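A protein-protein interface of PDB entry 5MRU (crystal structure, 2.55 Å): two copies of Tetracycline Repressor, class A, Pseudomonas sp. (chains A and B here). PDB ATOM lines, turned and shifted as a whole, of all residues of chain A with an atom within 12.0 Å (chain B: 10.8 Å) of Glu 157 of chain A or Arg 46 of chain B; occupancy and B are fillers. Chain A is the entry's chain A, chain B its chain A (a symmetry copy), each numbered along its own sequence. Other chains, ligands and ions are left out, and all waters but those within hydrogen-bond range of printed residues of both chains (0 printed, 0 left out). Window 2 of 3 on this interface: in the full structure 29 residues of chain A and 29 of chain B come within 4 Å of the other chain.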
ATOM      1  N   GLN A 149       3.953 -13.137 -21.597  1.00  0.00           N
ATOM      2  CA  GLN A 149       2.695 -13.878 -21.461  1.00  0.00           C
ATOM      3  C   GLN A 149       2.841 -15.122 -20.635  1.00  0.00           C
ATOM      4  O   GLN A 149       1.990 -15.424 -19.827  1.00  0.00           O
ATOM      5  CB  GLN A 149       2.134 -14.181 -22.820  1.00  0.00           C
ATOM      6  CG  GLN A 149       1.295 -13.031 -23.326  1.00  0.00           C
ATOM      7  CD  GLN A 149       0.702 -13.211 -24.704  1.00  0.00           C
ATOM      8  OE1 GLN A 149       1.199 -13.968 -25.524  1.00  0.00           O
ATOM      9  NE2 GLN A 149      -0.341 -12.468 -24.978  1.00  0.00           N
ATOM     10  N   ALA A 150       3.944 -15.820 -20.820  1.00  0.00           N
ATOM     11  CA  ALA A 150       4.279 -16.983 -20.051  1.00  0.00           C
ATOM     12  C   ALA A 150       4.619 -16.674 -18.595  1.00  0.00           C
ATOM     13  O   ALA A 150       4.175 -17.357 -17.694  1.00  0.00           O
ATOM     14  CB  ALA A 150       5.481 -17.617 -20.713  1.00  0.00           C
ATOM     15  N   GLY A 151       5.455 -15.664 -18.363  1.00  0.00           N
ATOM     16  CA  GLY A 151       5.831 -15.252 -17.011  1.00  0.00           C
ATOM     17  C   GLY A 151       4.582 -15.029 -16.182  1.00  0.00           C
ATOM     18  O   GLY A 151       4.478 -15.491 -15.036  1.00  0.00           O
ATOM     19  N   ASP A 152       3.627 -14.320 -16.792  1.00  0.00           N
ATOM     20  CA  ASP A 152       2.283 -14.129 -16.216  1.00  0.00           C
ATOM     21  C   ASP A 152       1.544 -15.465 -16.111  1.00  0.00           C
ATOM     22  O   ASP A 152       1.219 -15.882 -15.008  1.00  0.00           O
ATOM     23  CB  ASP A 152       1.473 -13.099 -17.035  1.00  0.00           C
ATOM     24  CG  ASP A 152       2.014 -11.656 -16.884  1.00  0.00           C
ATOM     25  OD1 ASP A 152       3.061 -11.445 -16.206  1.00  0.00           O
ATOM     26  OD2 ASP A 152       1.388 -10.730 -17.456  1.00  0.00           O
ATOM     27  N   SER A 153       1.321 -16.136 -17.253  1.00  0.00           N
ATOM     28  CA  SER A 153       0.686 -17.485 -17.324  1.00  0.00           C
ATOM     29  C   SER A 153       1.179 -18.548 -16.330  1.00  0.00           C
ATOM     30  O   SER A 153       0.393 -19.366 -15.897  1.00  0.00           O
ATOM     31  CB  SER A 153       0.819 -18.087 -18.738  1.00  0.00           C
ATOM     32  OG  SER A 153      -0.443 -18.304 -19.327  1.00  0.00           O
ATOM     33  N   GLU A 154       2.474 -18.537 -16.016  1.00  0.00           N
ATOM     34  CA  GLU A 154       3.129 -19.593 -15.227  1.00  0.00           C
ATOM     35  C   GLU A 154       3.183 -19.304 -13.731  1.00  0.00           C
ATOM     36  O   GLU A 154       3.629 -20.147 -12.946  1.00  0.00           O
ATOM     37  CB  GLU A 154       4.597 -19.807 -15.689  1.00  0.00           C
ATOM     38  CG  GLU A 154       4.879 -20.134 -17.169  1.00  0.00           C
ATOM     39  CD  GLU A 154       3.790 -20.927 -17.850  1.00  0.00           C
ATOM     40  OE1 GLU A 154       3.575 -20.675 -19.056  1.00  0.00           O
ATOM     41  OE2 GLU A 154       3.161 -21.788 -17.202  1.00  0.00           O
ATOM     42  N   SER A 155       2.758 -18.108 -13.341  1.00  0.00           N
ATOM     43  CA  SER A 155       2.894 -17.651 -11.951  1.00  0.00           C
ATOM     44  C   SER A 155       2.272 -18.554 -10.851  1.00  0.00           C
ATOM     45  O   SER A 155       2.651 -18.407  -9.691  1.00  0.00           O
ATOM     46  CB  SER A 155       2.375 -16.213 -11.827  1.00  0.00           C
ATOM     47  OG  SER A 155       3.325 -15.279 -12.327  1.00  0.00           O
ATOM     48  N   GLY A 156       1.324 -19.436 -11.224  1.00  0.00           N
ATOM     49  CA  GLY A 156       0.786 -20.536 -10.388  1.00  0.00           C
ATOM     50  C   GLY A 156       1.819 -21.419  -9.684  1.00  0.00           C
ATOM     51  O   GLY A 156       1.667 -21.686  -8.485  1.00  0.00           O
ATOM     52  N   GLU A 157       2.852 -21.884 -10.414  1.00  0.00           N
ATOM     53  CA  GLU A 157       4.110 -22.373  -9.777  1.00  0.00           C
ATOM     54  C   GLU A 157       5.158 -21.247  -9.445  1.00  0.00           C
ATOM     55  O   GLU A 157       5.330 -20.814  -8.268  1.00  0.00           O
ATOM     56  CB  GLU A 157       4.763 -23.480 -10.623  1.00  0.00           C
ATOM     57  N   LEU B   4      18.581 -30.137  -5.562  1.00  0.00           N
ATOM     58  CA  LEU B   4      18.549 -30.241  -7.059  1.00  0.00           C
ATOM     59  C   LEU B   4      17.532 -31.308  -7.530  1.00  0.00           C
ATOM     60  O   LEU B   4      16.362 -31.219  -7.140  1.00  0.00           O
ATOM     61  CB  LEU B   4      19.963 -30.499  -7.597  1.00  0.00           C
ATOM     62  N   GLN B   5      17.982 -32.284  -8.344  1.00  0.00           N
ATOM     63  CA  GLN B   5      17.143 -33.359  -8.973  1.00  0.00           C
ATOM     64  C   GLN B   5      18.005 -34.243  -9.913  1.00  0.00           C
ATOM     65  O   GLN B   5      18.779 -33.692 -10.696  1.00  0.00           O
ATOM     66  CB  GLN B   5      15.996 -32.771  -9.823  1.00  0.00           C
ATOM     67  CG  GLN B   5      14.845 -33.741 -10.091  1.00  0.00           C
ATOM     68  CD  GLN B   5      13.870 -33.796  -8.925  1.00  0.00           C
ATOM     69  OE1 GLN B   5      13.925 -34.689  -8.060  1.00  0.00           O
ATOM     70  NE2 GLN B   5      12.989 -32.799  -8.867  1.00  0.00           N
ATOM     71  N   VAL B   9      17.083 -38.943 -14.488  1.00  0.00           N
ATOM     72  CA  VAL B   9      15.689 -38.504 -14.621  1.00  0.00           C
ATOM     73  C   VAL B   9      15.541 -37.376 -15.648  1.00  0.00           C
ATOM     74  O   VAL B   9      14.583 -37.351 -16.429  1.00  0.00           O
ATOM     75  CB  VAL B   9      15.113 -38.041 -13.257  1.00  0.00           C
ATOM     76  CG1 VAL B   9      13.729 -37.431 -13.400  1.00  0.00           C
ATOM     77  CG2 VAL B   9      14.983 -39.210 -12.308  1.00  0.00           C
ATOM     78  N   THR B  26       4.179 -35.353 -19.697  1.00  0.00           N
ATOM     79  CA  THR B  26       3.721 -35.280 -18.312  1.00  0.00           C
ATOM     80  C   THR B  26       4.580 -36.151 -17.409  1.00  0.00           C
ATOM     81  O   THR B  26       5.251 -37.082 -17.839  1.00  0.00           O
ATOM     82  CB  THR B  26       2.287 -35.802 -18.154  1.00  0.00           C
ATOM     83  OG1 THR B  26       2.307 -37.228 -18.277  1.00  0.00           O
ATOM     84  CG2 THR B  26       1.372 -35.214 -19.200  1.00  0.00           C
ATOM     85  N   THR B  27       4.518 -35.868 -16.121  1.00  0.00           N
ATOM     86  CA  THR B  27       5.262 -36.639 -15.133  1.00  0.00           C
ATOM     87  C   THR B  27       4.811 -38.100 -15.096  1.00  0.00           C
ATOM     88  O   THR B  27       5.643 -38.978 -14.915  1.00  0.00           O
ATOM     89  CB  THR B  27       5.144 -35.996 -13.729  1.00  0.00           C
ATOM     90  OG1 THR B  27       3.775 -35.958 -13.336  1.00  0.00           O
ATOM     91  CG2 THR B  27       5.701 -34.552 -13.722  1.00  0.00           C
ATOM     92  N   LEU B  30       6.660 -39.530 -17.907  1.00  0.00           N
ATOM     93  CA  LEU B  30       8.061 -39.625 -17.533  1.00  0.00           C
ATOM     94  C   LEU B  30       8.328 -40.926 -16.755  1.00  0.00           C
ATOM     95  O   LEU B  30       9.262 -41.660 -17.088  1.00  0.00           O
ATOM     96  CB  LEU B  30       8.500 -38.405 -16.717  1.00  0.00           C
ATOM     97  CG  LEU B  30       9.973 -38.381 -16.265  1.00  0.00           C
ATOM     98  CD1 LEU B  30      10.942 -38.746 -17.397  1.00  0.00           C
ATOM     99  CD2 LEU B  30      10.329 -37.007 -15.695  1.00  0.00           C
ATOM    100  N   TYR B  42      14.792 -41.694  -5.949  1.00  0.00           N
ATOM    101  CA  TYR B  42      13.494 -41.038  -5.877  1.00  0.00           C
ATOM    102  C   TYR B  42      13.467 -39.666  -6.531  1.00  0.00           C
ATOM    103  O   TYR B  42      14.417 -38.905  -6.470  1.00  0.00           O
ATOM    104  CB  TYR B  42      13.093 -40.934  -4.417  1.00  0.00           C
ATOM    105  CG  TYR B  42      11.762 -40.313  -4.157  1.00  0.00           C
ATOM    106  CD1 TYR B  42      10.603 -41.072  -4.145  1.00  0.00           C
ATOM    107  CD2 TYR B  42      11.662 -38.975  -3.866  1.00  0.00           C
ATOM    108  CE1 TYR B  42       9.365 -40.503  -3.870  1.00  0.00           C
ATOM    109  CE2 TYR B  42      10.435 -38.384  -3.610  1.00  0.00           C
ATOM    110  CZ  TYR B  42       9.286 -39.152  -3.609  1.00  0.00           C
ATOM    111  OH  TYR B  42       8.080 -38.544  -3.344  1.00  0.00           O
ATOM    112  N   TRP B  43      12.356 -39.346  -7.167  1.00  0.00           N
ATOM    113  CA  TRP B  43      12.218 -38.028  -7.738  1.00  0.00           C
ATOM    114  C   TRP B  43      10.783 -37.561  -7.725  1.00  0.00           C
ATOM    115  O   TRP B  43       9.865 -38.357  -7.831  1.00  0.00           O
ATOM    116  CB  TRP B  43      12.718 -38.013  -9.179  1.00  0.00           C
ATOM    117  CG  TRP B  43      11.939 -38.914 -10.045  1.00  0.00           C
ATOM    118  CD1 TRP B  43      12.121 -40.264 -10.199  1.00  0.00           C
ATOM    119  CD2 TRP B  43      10.817 -38.563 -10.851  1.00  0.00           C
ATOM    120  NE1 TRP B  43      11.185 -40.764 -11.072  1.00  0.00           N
ATOM    121  CE2 TRP B  43      10.382 -39.740 -11.495  1.00  0.00           C
ATOM    122  CE3 TRP B  43      10.131 -37.373 -11.082  1.00  0.00           C
ATOM    123  CZ2 TRP B  43       9.297 -39.766 -12.346  1.00  0.00           C
ATOM    124  CZ3 TRP B  43       9.047 -37.386 -11.964  1.00  0.00           C
ATOM    125  CH2 TRP B  43       8.643 -38.582 -12.584  1.00  0.00           C
ATOM    126  N   HIS B  44      10.603 -36.251  -7.630  1.00  0.00           N
ATOM    127  CA  HIS B  44       9.291 -35.689  -7.646  1.00  0.00           C
ATOM    128  C   HIS B  44       9.322 -34.273  -8.173  1.00  0.00           C
ATOM    129  O   HIS B  44      10.162 -33.500  -7.774  1.00  0.00           O
ATOM    130  CB  HIS B  44       8.648 -35.696  -6.251  1.00  0.00           C
ATOM    131  CG  HIS B  44       7.306 -35.064  -6.254  1.00  0.00           C
ATOM    132  ND1 HIS B  44       6.224 -35.664  -6.851  1.00  0.00           N
ATOM    133  CD2 HIS B  44       6.897 -33.827  -5.883  1.00  0.00           C
ATOM    134  CE1 HIS B  44       5.192 -34.844  -6.819  1.00  0.00           C
ATOM    135  NE2 HIS B  44       5.571 -33.725  -6.225  1.00  0.00           N
ATOM    136  N   PHE B  45       8.385 -33.917  -9.042  1.00  0.00           N
ATOM    137  CA  PHE B  45       8.274 -32.521  -9.432  1.00  0.00           C
ATOM    138  C   PHE B  45       7.014 -31.866  -8.858  1.00  0.00           C
ATOM    139  O   PHE B  45       5.934 -32.463  -8.859  1.00  0.00           O
ATOM    140  CB  PHE B  45       8.338 -32.394 -10.946  1.00  0.00           C
ATOM    141  CG  PHE B  45       9.676 -32.771 -11.515  1.00  0.00           C
ATOM    142  CD1 PHE B  45      10.726 -31.882 -11.486  1.00  0.00           C
ATOM    143  CD2 PHE B  45       9.879 -34.044 -12.083  1.00  0.00           C
ATOM    144  CE1 PHE B  45      11.958 -32.241 -12.023  1.00  0.00           C
ATOM    145  CE2 PHE B  45      11.095 -34.405 -12.633  1.00  0.00           C
ATOM    146  CZ  PHE B  45      12.142 -33.506 -12.593  1.00  0.00           C
ATOM    147  N   ARG B  46       7.169 -30.651  -8.350  1.00  0.00           N
ATOM    148  CA  ARG B  46       6.054 -29.985  -7.713  1.00  0.00           C
ATOM    149  C   ARG B  46       4.882 -29.866  -8.719  1.00  0.00           C
ATOM    150  O   ARG B  46       3.735 -29.967  -8.364  1.00  0.00           O
ATOM    151  CB  ARG B  46       6.522 -28.645  -7.121  1.00  0.00           C
ATOM    152  CG  ARG B  46       5.418 -27.699  -6.689  1.00  0.00           C
ATOM    153  CD  ARG B  46       5.877 -26.803  -5.546  1.00  0.00           C
ATOM    154  NE  ARG B  46       4.937 -25.714  -5.249  1.00  0.00           N
ATOM    155  CZ  ARG B  46       4.746 -24.641  -6.029  1.00  0.00           C
ATOM    156  NH1 ARG B  46       5.417 -24.486  -7.186  1.00  0.00           N
ATOM    157  NH2 ARG B  46       3.869 -23.707  -5.654  1.00  0.00           N
ATOM    158  N   ASN B  47       5.183 -29.709  -9.992  1.00  0.00           N
ATOM    159  CA  ASN B  47       4.171 -29.702 -11.033  1.00  0.00           C
ATOM    160  C   ASN B  47       4.879 -29.640 -12.361  1.00  0.00           C
ATOM    161  O   ASN B  47       6.110 -29.539 -12.424  1.00  0.00           O
ATOM    162  CB  ASN B  47       3.227 -28.503 -10.896  1.00  0.00           C
ATOM    163  CG  ASN B  47       3.956 -27.191 -10.577  1.00  0.00           C
ATOM    164  OD1 ASN B  47       5.042 -26.907 -11.092  1.00  0.00           O
ATOM    165  ND2 ASN B  47       3.342 -26.381  -9.736  1.00  0.00           N
ATOM    166  N   LYS B  48       4.103 -29.675 -13.434  1.00  0.00           N
ATOM    167  CA  LYS B  48       4.673 -29.689 -14.754  1.00  0.00           C
ATOM    168  C   LYS B  48       5.618 -28.519 -14.959  1.00  0.00           C
ATOM    169  O   LYS B  48       6.683 -28.656 -15.513  1.00  0.00           O
ATOM    170  CB  LYS B  48       3.570 -29.687 -15.792  1.00  0.00           C
ATOM    171  CG  LYS B  48       4.087 -30.082 -17.161  1.00  0.00           C
ATOM    172  CD  LYS B  48       3.006 -30.099 -18.246  1.00  0.00           C
ATOM    173  CE  LYS B  48       3.659 -30.042 -19.624  1.00  0.00           C
ATOM    174  NZ  LYS B  48       2.688 -30.406 -20.681  1.00  0.00           N
ATOM    175  N   ARG B  49       5.241 -27.355 -14.469  1.00  0.00           N
ATOM    176  CA  ARG B  49       5.974 -26.154 -14.743  1.00  0.00           C
ATOM    177  C   ARG B  49       7.369 -26.271 -14.189  1.00  0.00           C
ATOM    178  O   ARG B  49       8.348 -25.760 -14.763  1.00  0.00           O
ATOM    179  CB  ARG B  49       5.245 -24.987 -14.096  1.00  0.00           C
ATOM    180  CG  ARG B  49       5.782 -23.653 -14.580  1.00  0.00           C
ATOM    181  CD  ARG B  49       5.961 -23.596 -16.094  1.00  0.00           C
ATOM    182  NE  ARG B  49       7.350 -23.648 -16.508  1.00  0.00           N
ATOM    183  CZ  ARG B  49       7.804 -23.345 -17.731  1.00  0.00           C
ATOM    184  NH1 ARG B  49       7.009 -22.968 -18.734  1.00  0.00           N
ATOM    185  NH2 ARG B  49       9.104 -23.428 -17.940  1.00  0.00           N
ATOM    186  N   ALA B  50       7.429 -26.949 -13.051  1.00  0.00           N
ATOM    187  CA  ALA B  50       8.669 -27.238 -12.348  1.00  0.00           C
ATOM    188  C   ALA B  50       9.529 -28.183 -13.185  1.00  0.00           C
ATOM    189  O   ALA B  50      10.744 -28.018 -13.242  1.00  0.00           O
ATOM    190  CB  ALA B  50       8.365 -27.869 -11.003  1.00  0.00           C
ATOM    191  N   LEU B  51       8.905 -29.172 -13.812  1.00  0.00           N
ATOM    192  CA  LEU B  51       9.609 -30.039 -14.749  1.00  0.00           C
ATOM    193  C   LEU B  51      10.201 -29.244 -15.907  1.00  0.00           C
ATOM    194  O   LEU B  51      11.373 -29.447 -16.266  1.00  0.00           O
ATOM    195  CB  LEU B  51       8.693 -31.150 -15.304  1.00  0.00           C
ATOM    196  CG  LEU B  51       9.305 -32.092 -16.354  1.00  0.00           C
ATOM    197  CD1 LEU B  51      10.702 -32.608 -15.995  1.00  0.00           C
ATOM    198  CD2 LEU B  51       8.359 -33.245 -16.659  1.00  0.00           C
ATOM    199  N   LEU B  52       9.401 -28.345 -16.479  1.00  0.00           N
ATOM    200  CA  LEU B  52       9.857 -27.570 -17.609  1.00  0.00           C
ATOM    201  C   LEU B  52      10.900 -26.529 -17.138  1.00  0.00           C
ATOM    202  O   LEU B  52      11.776 -26.136 -17.897  1.00  0.00           O
ATOM    203  CB  LEU B  52       8.676 -26.902 -18.312  1.00  0.00           C
ATOM    204  CG  LEU B  52       7.548 -27.829 -18.783  1.00  0.00           C
ATOM    205  CD1 LEU B  52       6.424 -27.068 -19.480  1.00  0.00           C
ATOM    206  CD2 LEU B  52       8.074 -28.900 -19.696  1.00  0.00           C
ATOM    207  N   ASP B  53      10.830 -26.066 -15.899  1.00  0.00           N
ATOM    208  CA  ASP B  53      11.908 -25.175 -15.431  1.00  0.00           C
ATOM    209  C   ASP B  53      13.240 -25.902 -15.349  1.00  0.00           C
ATOM    210  O   ASP B  53      14.262 -25.377 -15.785  1.00  0.00           O
ATOM    211  CB  ASP B  53      11.563 -24.494 -14.121  1.00  0.00           C
ATOM    212  CG  ASP B  53      10.573 -23.361 -14.319  1.00  0.00           C
ATOM    213  OD1 ASP B  53      10.205 -23.062 -15.479  1.00  0.00           O
ATOM    214  OD2 ASP B  53      10.145 -22.758 -13.301  1.00  0.00           O
ATOM    215  N   ALA B  54      13.214 -27.130 -14.836  1.00  0.00           N
ATOM    216  CA  ALA B  54      14.408 -27.967 -14.781  1.00  0.00           C
ATOM    217  C   ALA B  54      14.936 -28.271 -16.207  1.00  0.00           C
ATOM    218  O   ALA B  54      16.143 -28.173 -16.474  1.00  0.00           O
ATOM    219  CB  ALA B  54      14.122 -29.249 -14.015  1.00  0.00           C
ATOM    220  N   GLY B 102       9.366 -17.212 -20.037  1.00  0.00           N
ATOM    221  CA  GLY B 102       8.917 -16.996 -18.695  1.00  0.00           C
ATOM    222  C   GLY B 102       9.828 -17.532 -17.620  1.00  0.00           C
ATOM    223  O   GLY B 102       9.538 -17.353 -16.466  1.00  0.00           O
ATOM    224  N   THR B 103      10.927 -18.182 -17.958  1.00  0.00           N
ATOM    225  CA  THR B 103      11.811 -18.655 -16.908  1.00  0.00           C
ATOM    226  C   THR B 103      12.674 -17.484 -16.508  1.00  0.00           C
ATOM    227  O   THR B 103      12.827 -16.531 -17.263  1.00  0.00           O
ATOM    228  CB  THR B 103      12.714 -19.858 -17.300  1.00  0.00           C
ATOM    229  OG1 THR B 103      13.595 -19.506 -18.373  1.00  0.00           O
ATOM    230  CG2 THR B 103      11.890 -21.091 -17.676  1.00  0.00           C
ATOM    231  N   ARG B 104      13.179 -17.532 -15.288  1.00  0.00           N
ATOM    232  CA  ARG B 104      14.068 -16.500 -14.779  1.00  0.00           C
ATOM    233  C   ARG B 104      15.294 -17.219 -14.283  1.00  0.00           C
ATOM    234  O   ARG B 104      15.183 -18.204 -13.546  1.00  0.00           O
ATOM    235  CB  ARG B 104      13.404 -15.670 -13.668  1.00  0.00           C
ATOM    236  CG  ARG B 104      12.735 -14.379 -14.153  1.00  0.00           C
ATOM    237  CD  ARG B 104      11.972 -14.601 -15.465  1.00  0.00           C
ATOM    238  NE  ARG B 104      11.064 -13.574 -15.996  1.00  0.00           N
ATOM    239  CZ  ARG B 104      10.995 -12.284 -15.659  1.00  0.00           C
ATOM    240  NH1 ARG B 104      11.772 -11.726 -14.727  1.00  0.00           N
ATOM    241  NH2 ARG B 104      10.084 -11.534 -16.272  1.00  0.00           N
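Among the printed residues, merely in contact across the chains: Glu 157 of chain A with Asn 47 of chain B (3.3 Å), Glu 154 of chain A with Arg 49 of chain B (3.5 Å), Glu 157 of chain A with Arg 46 of chain B (3.6 Å), Gly 151 of chain A with Gly 102 of chain B (3.7 Å), Glu 157 of chain A with Arg 49 of chain B (3.8 Å) and Ala 150 of chain A with Gly 102 of chain B (3.96 Å).
No position is printed for both chains.
The backbone NH (N) of Ala 50 of chain B is in hydrogen-bond range of the side-chain amide oxygen (OD1) of Asn 47 of chain B, 3.1 Å away.
OD1 of Asp 53 of chain B lies within salt-bridge range of NH2 of Arg 49 of chain B (2.7 Å).
OG of Ser 155 of chain A lies within hydrogen-bond range of O of Gly 151 of chain A (3.0 Å).
The backbone NH of Arg 49 of chain B lies close to the side-chain amide oxygen of Asn 47 of chain B (3.4 Å).
Of the 22 printed residues of chain B, 4 touch a printed residue of chain A.
Printed residues of chain B that touch a printed residue of chain A: Arg 46, Asn 47, Arg 49 and Gly 102.
Among the printed residues, no Asp or Glu carboxylate lies within 4 Å of a Lys or Arg side-chain nitrogen of the other chain.
Of the printed residues of chain B, Gly 151 of chain A touches Gly 102.
Gly 156 of chain A touches none of the printed residues of chain B.
Of chain B, only Arg 46 (3.6 Å), Asn 47 (3.3 Å) and Arg 49 (3.8 Å) come within 4 Å of Glu 157 of chain A.
No residue of chain A comes within 4 Å of Phe 45 of chain B.
Arg 46 of chain B touches one residue of chain A.
Of chain A, only Glu 157 (3.3 Å) comes within 4 Å of Asn 47 of chain B.
Printed residues of chain A within 4 Å of Arg 49 of chain B: Glu 154 (3.5 Å) and Glu 157 (3.8 Å).
Ala 50 of chain B touches none of the printed residues of chain A.
Printed residues of chain A within 4 Å of Gly 102 of chain B: Ala 150 (3.96 Å) and Gly 151 (3.7 Å).
Arg 104 of chain B touches none of the printed residues of chain A.
The nearest residue of chain A that does not touch Arg 46 of chain B is Gly 156 of chain A (4.1 Å).
The nearest printed residue of chain B that does not touch Ala 150 of chain A is Arg 49 of chain B (5.9 Å).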
